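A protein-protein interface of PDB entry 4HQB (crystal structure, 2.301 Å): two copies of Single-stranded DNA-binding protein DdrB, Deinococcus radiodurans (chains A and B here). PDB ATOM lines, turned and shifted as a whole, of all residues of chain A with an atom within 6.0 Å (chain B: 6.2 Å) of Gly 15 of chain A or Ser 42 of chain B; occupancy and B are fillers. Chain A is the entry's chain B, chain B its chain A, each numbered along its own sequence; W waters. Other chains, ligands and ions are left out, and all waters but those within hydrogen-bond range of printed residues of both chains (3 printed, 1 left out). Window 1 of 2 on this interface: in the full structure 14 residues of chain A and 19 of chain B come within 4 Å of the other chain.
OE1 of Glu 9 of chain B is in salt-bridge range of NH1 of Arg 17 of chain A (3.5 Å).
The side-chain hydroxyl (OG) of Ser 42 of chain B lies within hydrogen-bond range of the backbone NH (N) of Arg 17 of chain A.
O of Gly 15 of chain A sits close to O of Ser 42 of chain B (3.5 Å).
The backbone carbonyl oxygen (O) of Glu 9 of chain B sits at hydrogen-bond distance from the side-chain hydroxyl (OG) of Ser 42 of chain B (2.8 Å).
OG1 of Thr 12 of chain A lies close to N of Leu 14 of chain A (3.1 Å).
OG1 of Thr 12 of chain A lies within hydrogen-bond range of N of Gly 15 of chain A, 3.4 Å away.
The side-chain hydroxyl of Thr 12 of chain A sits at hydrogen-bond distance from the backbone NH of Ala 16 of chain A (3.1 Å).
Tyr 50 of chain B touches Leu 14 of chain A.
Gly 15 of chain A touches Gly 43 of chain B.
CB of Ala 16 of chain A touches CD1 of Ile 8 of chain B, 3.9 Å away.
OE1 of Gln 32 of chain B touches CB of Ala 16 of chain A (3.9 Å).
CA of Ala 16 of chain A touches OG of Ser 42 of chain B, 3.4 Å away.
O of Arg 17 of chain A touches CA of Ile 8 of chain B (3.3 Å).
CG of Arg 17 of chain A touches CA of Gly 43 of chain B, at 3.7 Å.
Printed residues of chain B that touch a printed residue of chain A: Ile 8, Glu 9, Gln 32, Ser 42, Gly 43 and Tyr 50.
Hydrophobic or aromatic side chains of chain B within 4 Å of the printed part of chain A: Ile 8 and Tyr 50.
Among the printed residues, 10 pairs touch across the chains.
Of the printed residues of chain B, Gly 15 of chain A touches Ser 42 and Gly 43.
Of the printed residues of chain A, Ile 8 of chain B touches Ala 16 (3.9 Å) and Arg 17 (3.3 Å).
Of the printed residues of chain A, Glu 9 of chain B touches Arg 17 (2.4 Å).
Of chain A, only Gly 15 (3.5 Å), Ala 16 (3.4 Å) and Arg 17 (3.0 Å) come within 4 Å of Ser 42 of chain B.
Of the printed residues of chain A, Gly 43 of chain B touches Gly 15 (3.5 Å) and Arg 17 (3.7 Å).
Of the printed residues of chain A, Tyr 50 of chain B touches Leu 14 (3.1 Å).
Ile 65 of chain B touches none of the printed residues of chain A.
The nearest printed residue of chain A that does not touch Ile 8 of chain B is Val 18 of chain A (4.3 Å).
Position printed for both chains: 11.
Of the 10 pairs that touch across the chains among the printed residues, none has its exchanged pair printed and touching as well.
Water W1 bridges O of Gly 15 of chain A (2.7 Å) and N of Glu 44 of chain B (3.0 Å).
Water W3 bridges the side-chain amide oxygen of Gln 32 of chain B (2.8 Å) and the side-chain hydroxyl of Thr 12 of chain A (2.8 Å).
Water W2 lies within hydrogen-bond range of O of Leu 14 of chain A (2.8 Å), O of Ser 42 of chain B (3.0 Å) and NE2 of Gln 32 of chain B (3.3 Å).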
ATOM      1  N   ILE A  11     -19.955  30.331   0.198  1.00  0.00           N
ATOM      2  CA  ILE A  11     -18.618  30.936   0.228  1.00  0.00           C
ATOM      3  C   ILE A  11     -18.665  31.874   1.408  1.00  0.00           C
ATOM      4  O   ILE A  11     -19.492  32.785   1.413  1.00  0.00           O
ATOM      5  CB  ILE A  11     -18.325  31.819  -1.002  1.00  0.00           C
ATOM      6  CG1 ILE A  11     -18.439  31.030  -2.312  1.00  0.00           C
ATOM      7  CG2 ILE A  11     -16.956  32.508  -0.856  1.00  0.00           C
ATOM      8  CD1 ILE A  11     -17.533  29.864  -2.390  1.00  0.00           C
ATOM      9  N   THR A  12     -17.814  31.664   2.413  1.00  0.00           N
ATOM     10  CA  THR A  12     -17.911  32.470   3.622  1.00  0.00           C
ATOM     11  C   THR A  12     -17.426  33.894   3.386  1.00  0.00           C
ATOM     12  O   THR A  12     -16.996  34.244   2.291  1.00  0.00           O
ATOM     13  CB  THR A  12     -17.095  31.893   4.778  1.00  0.00           C
ATOM     14  OG1 THR A  12     -15.695  31.926   4.440  1.00  0.00           O
ATOM     15  CG2 THR A  12     -17.559  30.464   5.107  1.00  0.00           C
ATOM     16  N   ASP A  13     -17.481  34.710   4.429  1.00  0.00           N
ATOM     17  CA  ASP A  13     -16.916  36.052   4.351  1.00  0.00           C
ATOM     18  C   ASP A  13     -15.391  36.013   4.150  1.00  0.00           C
ATOM     19  O   ASP A  13     -14.797  37.027   3.779  1.00  0.00           O
ATOM     20  CB  ASP A  13     -17.303  36.917   5.572  1.00  0.00           C
ATOM     21  CG  ASP A  13     -16.807  36.341   6.921  1.00  0.00           C
ATOM     22  OD1 ASP A  13     -16.770  35.103   7.103  1.00  0.00           O
ATOM     23  OD2 ASP A  13     -16.487  37.143   7.827  1.00  0.00           O
ATOM     24  N   LEU A  14     -14.763  34.856   4.394  1.00  0.00           N
ATOM     25  CA  LEU A  14     -13.304  34.725   4.197  1.00  0.00           C
ATOM     26  C   LEU A  14     -12.956  33.913   2.958  1.00  0.00           C
ATOM     27  O   LEU A  14     -11.813  33.492   2.785  1.00  0.00           O
ATOM     28  CB  LEU A  14     -12.605  34.119   5.426  1.00  0.00           C
ATOM     29  CG  LEU A  14     -12.230  35.089   6.547  1.00  0.00           C
ATOM     30  CD1 LEU A  14     -12.729  36.511   6.262  1.00  0.00           C
ATOM     31  CD2 LEU A  14     -12.766  34.598   7.873  1.00  0.00           C
ATOM     32  N   GLY A  15     -13.946  33.684   2.107  1.00  0.00           N
ATOM     33  CA  GLY A  15     -13.720  32.940   0.882  1.00  0.00           C
ATOM     34  C   GLY A  15     -13.830  31.416   0.972  1.00  0.00           C
ATOM     35  O   GLY A  15     -13.834  30.751  -0.056  1.00  0.00           O
ATOM     36  N   ALA A  16     -13.918  30.866   2.182  1.00  0.00           N
ATOM     37  CA  ALA A  16     -13.987  29.406   2.372  1.00  0.00           C
ATOM     38  C   ALA A  16     -15.209  28.756   1.697  1.00  0.00           C
ATOM     39  O   ALA A  16     -16.308  29.318   1.701  1.00  0.00           O
ATOM     40  CB  ALA A  16     -13.951  29.059   3.850  1.00  0.00           C
ATOM     41  N   ARG A  17     -15.001  27.585   1.099  1.00  0.00           N
ATOM     42  CA  ARG A  17     -16.099  26.795   0.537  1.00  0.00           C
ATOM     43  C   ARG A  17     -16.649  25.871   1.613  1.00  0.00           C
ATOM     44  O   ARG A  17     -16.040  24.861   1.967  1.00  0.00           O
ATOM     45  CB  ARG A  17     -15.655  25.968  -0.678  1.00  0.00           C
ATOM     46  CG  ARG A  17     -15.000  26.769  -1.772  1.00  0.00           C
ATOM     47  CD  ARG A  17     -14.673  25.911  -3.017  1.00  0.00           C
ATOM     48  NE  ARG A  17     -15.733  26.008  -4.021  1.00  0.00           N
ATOM     49  CZ  ARG A  17     -16.646  25.071  -4.236  1.00  0.00           C
ATOM     50  NH1 ARG A  17     -16.617  23.949  -3.533  1.00  0.00           N
ATOM     51  NH2 ARG A  17     -17.578  25.246  -5.163  1.00  0.00           N
ATOM     52  N   VAL A  18     -17.818  26.227   2.117  1.00  0.00           N
ATOM     53  CA  VAL A  18     -18.369  25.586   3.292  1.00  0.00           C
ATOM     54  C   VAL A  18     -19.789  25.079   3.026  1.00  0.00           C
ATOM     55  O   VAL A  18     -20.593  25.765   2.389  1.00  0.00           O
ATOM     56  CB  VAL A  18     -18.364  26.591   4.458  1.00  0.00           C
ATOM     57  CG1 VAL A  18     -19.034  26.026   5.671  1.00  0.00           C
ATOM     58  CG2 VAL A  18     -16.922  27.020   4.785  1.00  0.00           C
ATOM     59  N   ILE B   8     -15.902  21.723   5.077  1.00  0.00           N
ATOM     60  CA  ILE B   8     -15.117  22.704   4.336  1.00  0.00           C
ATOM     61  C   ILE B   8     -14.225  22.055   3.278  1.00  0.00           C
ATOM     62  O   ILE B   8     -13.510  21.094   3.565  1.00  0.00           O
ATOM     63  CB  ILE B   8     -14.285  23.593   5.279  1.00  0.00           C
ATOM     64  CG1 ILE B   8     -13.411  24.552   4.473  1.00  0.00           C
ATOM     65  CG2 ILE B   8     -13.441  22.746   6.240  1.00  0.00           C
ATOM     66  CD1 ILE B   8     -12.808  25.668   5.343  1.00  0.00           C
ATOM     67  N   GLU B   9     -14.301  22.571   2.053  1.00  0.00           N
ATOM     68  CA  GLU B   9     -13.503  22.065   0.937  1.00  0.00           C
ATOM     69  C   GLU B   9     -12.150  22.776   0.807  1.00  0.00           C
ATOM     70  O   GLU B   9     -12.074  24.000   0.673  1.00  0.00           O
ATOM     71  CB  GLU B   9     -14.258  22.197  -0.385  1.00  0.00           C
ATOM     72  CG  GLU B   9     -15.319  21.152  -0.664  1.00  0.00           C
ATOM     73  CD  GLU B   9     -15.874  21.291  -2.081  1.00  0.00           C
ATOM     74  OE1 GLU B   9     -16.880  20.621  -2.413  1.00  0.00           O
ATOM     75  OE2 GLU B   9     -15.294  22.080  -2.866  1.00  0.00           O
ATOM     76  N   PHE B  10     -11.089  21.985   0.817  1.00  0.00           N
ATOM     77  CA  PHE B  10      -9.733  22.479   0.710  1.00  0.00           C
ATOM     78  C   PHE B  10      -9.086  22.037  -0.597  1.00  0.00           C
ATOM     79  O   PHE B  10      -9.524  21.078  -1.231  1.00  0.00           O
ATOM     80  CB  PHE B  10      -8.897  21.901   1.846  1.00  0.00           C
ATOM     81  CG  PHE B  10      -9.143  22.533   3.177  1.00  0.00           C
ATOM     82  CD1 PHE B  10      -8.727  23.853   3.431  1.00  0.00           C
ATOM     83  CD2 PHE B  10      -9.722  21.807   4.203  1.00  0.00           C
ATOM     84  CE1 PHE B  10      -8.925  24.441   4.667  1.00  0.00           C
ATOM     85  CE2 PHE B  10      -9.908  22.394   5.462  1.00  0.00           C
ATOM     86  CZ  PHE B  10      -9.516  23.715   5.682  1.00  0.00           C
ATOM     87  N   ILE B  11      -8.034  22.750  -0.984  1.00  0.00           N
ATOM     88  CA  ILE B  11      -7.073  22.289  -1.981  1.00  0.00           C
ATOM     89  C   ILE B  11      -5.751  22.164  -1.239  1.00  0.00           C
ATOM     90  O   ILE B  11      -5.259  23.155  -0.696  1.00  0.00           O
ATOM     91  CB  ILE B  11      -6.892  23.302  -3.147  1.00  0.00           C
ATOM     92  CG1 ILE B  11      -8.199  23.528  -3.923  1.00  0.00           C
ATOM     93  CG2 ILE B  11      -5.769  22.859  -4.066  1.00  0.00           C
ATOM     94  CD1 ILE B  11      -8.773  22.301  -4.576  1.00  0.00           C
ATOM     95  N   GLN B  32      -9.399  26.183   9.434  1.00  0.00           N
ATOM     96  CA  GLN B  32      -8.704  26.864   8.340  1.00  0.00           C
ATOM     97  C   GLN B  32      -7.252  27.121   8.713  1.00  0.00           C
ATOM     98  O   GLN B  32      -6.350  26.859   7.922  1.00  0.00           O
ATOM     99  CB  GLN B  32      -9.390  28.187   7.978  1.00  0.00           C
ATOM    100  CG  GLN B  32     -10.594  28.013   7.060  1.00  0.00           C
ATOM    101  CD  GLN B  32     -11.306  29.319   6.760  1.00  0.00           C
ATOM    102  OE1 GLN B  32     -12.345  29.616   7.349  1.00  0.00           O
ATOM    103  NE2 GLN B  32     -10.752  30.107   5.840  1.00  0.00           N
ATOM    104  N   TRP B  40      -2.595  24.481   2.872  1.00  0.00           N
ATOM    105  CA  TRP B  40      -3.920  24.214   2.298  1.00  0.00           C
ATOM    106  C   TRP B  40      -4.725  25.497   2.162  1.00  0.00           C
ATOM    107  O   TRP B  40      -4.708  26.345   3.052  1.00  0.00           O
ATOM    108  CB  TRP B  40      -4.734  23.206   3.133  1.00  0.00           C
ATOM    109  CG  TRP B  40      -4.147  21.815   3.227  1.00  0.00           C
ATOM    110  CD1 TRP B  40      -2.838  21.448   3.035  1.00  0.00           C
ATOM    111  CD2 TRP B  40      -4.864  20.608   3.538  1.00  0.00           C
ATOM    112  NE1 TRP B  40      -2.703  20.090   3.208  1.00  0.00           N
ATOM    113  CE2 TRP B  40      -3.924  19.552   3.526  1.00  0.00           C
ATOM    114  CE3 TRP B  40      -6.212  20.318   3.819  1.00  0.00           C
ATOM    115  CZ2 TRP B  40      -4.291  18.216   3.782  1.00  0.00           C
ATOM    116  CZ3 TRP B  40      -6.576  18.994   4.087  1.00  0.00           C
ATOM    117  CH2 TRP B  40      -5.612  17.962   4.066  1.00  0.00           C
ATOM    118  N   THR B  41      -5.451  25.628   1.054  1.00  0.00           N
ATOM    119  CA  THR B  41      -6.365  26.758   0.881  1.00  0.00           C
ATOM    120  C   THR B  41      -7.804  26.313   0.615  1.00  0.00           C
ATOM    121  O   THR B  41      -8.045  25.220   0.060  1.00  0.00           O
ATOM    122  CB  THR B  41      -5.914  27.657  -0.280  1.00  0.00           C
ATOM    123  OG1 THR B  41      -5.883  26.884  -1.489  1.00  0.00           O
ATOM    124  CG2 THR B  41      -4.513  28.226   0.002  1.00  0.00           C
ATOM    125  N   SER B  42      -8.746  27.176   0.991  1.00  0.00           N
ATOM    126  CA  SER B  42     -10.168  26.945   0.722  1.00  0.00           C
ATOM    127  C   SER B  42     -10.757  28.084  -0.101  1.00  0.00           C
ATOM    128  O   SER B  42     -10.765  29.220   0.342  1.00  0.00           O
ATOM    129  CB  SER B  42     -10.957  26.820   2.033  1.00  0.00           C
ATOM    130  OG  SER B  42     -12.315  26.522   1.758  1.00  0.00           O
ATOM    131  N   GLY B  43     -11.274  27.775  -1.283  1.00  0.00           N
ATOM    132  CA  GLY B  43     -11.866  28.788  -2.128  1.00  0.00           C
ATOM    133  C   GLY B  43     -10.845  29.495  -3.006  1.00  0.00           C
ATOM    134  O   GLY B  43      -9.682  29.126  -3.053  1.00  0.00           O
ATOM    135  N   GLU B  44     -11.292  30.505  -3.735  1.00  0.00           N
ATOM    136  CA  GLU B  44     -10.368  31.311  -4.514  1.00  0.00           C
ATOM    137  C   GLU B  44     -10.110  32.594  -3.771  1.00  0.00           C
ATOM    138  O   GLU B  44     -10.851  32.953  -2.863  1.00  0.00           O
ATOM    139  CB  GLU B  44     -10.921  31.624  -5.905  1.00  0.00           C
ATOM    140  CG  GLU B  44     -10.555  30.562  -6.929  1.00  0.00           C
ATOM    141  CD  GLU B  44      -9.050  30.245  -6.939  1.00  0.00           C
ATOM    142  OE1 GLU B  44      -8.219  31.189  -7.050  1.00  0.00           O
ATOM    143  OE2 GLU B  44      -8.702  29.045  -6.826  1.00  0.00           O
ATOM    144  N   PRO B  46     -10.706  36.167  -3.308  1.00  0.00           N
ATOM    145  CA  PRO B  46     -11.785  37.107  -3.658  1.00  0.00           C
ATOM    146  C   PRO B  46     -11.328  38.171  -4.640  1.00  0.00           C
ATOM    147  O   PRO B  46     -10.118  38.413  -4.788  1.00  0.00           O
ATOM    148  CB  PRO B  46     -12.130  37.775  -2.322  1.00  0.00           C
ATOM    149  CG  PRO B  46     -11.812  36.753  -1.300  1.00  0.00           C
ATOM    150  CD  PRO B  46     -10.625  35.949  -1.853  1.00  0.00           C
ATOM    151  N   TYR B  50      -8.401  39.427  -0.413  1.00  0.00           N
ATOM    152  CA  TYR B  50      -9.141  39.435   0.844  1.00  0.00           C
ATOM    153  C   TYR B  50      -9.075  40.844   1.443  1.00  0.00           C
ATOM    154  O   TYR B  50      -8.030  41.534   1.347  1.00  0.00           O
ATOM    155  CB  TYR B  50      -8.557  38.426   1.829  1.00  0.00           C
ATOM    156  CG  TYR B  50      -8.521  36.993   1.338  1.00  0.00           C
ATOM    157  CD1 TYR B  50      -9.607  36.144   1.532  1.00  0.00           C
ATOM    158  CD2 TYR B  50      -7.395  36.486   0.685  1.00  0.00           C
ATOM    159  CE1 TYR B  50      -9.575  34.829   1.087  1.00  0.00           C
ATOM    160  CE2 TYR B  50      -7.352  35.183   0.233  1.00  0.00           C
ATOM    161  CZ  TYR B  50      -8.449  34.357   0.438  1.00  0.00           C
ATOM    162  OH  TYR B  50      -8.421  33.061  -0.005  1.00  0.00           O
ATOM    163  N   ILE B  65      -5.307  31.945   5.577  1.00  0.00           N
ATOM    164  CA  ILE B  65      -5.623  31.834   4.156  1.00  0.00           C
ATOM    165  C   ILE B  65      -4.562  31.005   3.462  1.00  0.00           C
ATOM    166  O   ILE B  65      -4.367  31.106   2.248  1.00  0.00           O
ATOM    167  CB  ILE B  65      -5.716  33.206   3.485  1.00  0.00           C
ATOM    168  CG1 ILE B  65      -4.407  33.992   3.669  1.00  0.00           C
ATOM    169  CG2 ILE B  65      -6.916  33.995   4.058  1.00  0.00           C
ATOM    170  CD1 ILE B  65      -4.137  35.002   2.554  1.00  0.00           C
HETATM  171  O   HOH W   1     -13.823  31.573  -2.605  1.00  0.00           O
HETATM  172  O   HOH W   2     -10.446  31.006   2.717  1.00  0.00           O
HETATM  173  O   HOH W   3     -14.464  31.298   6.842  1.00  0.00           O
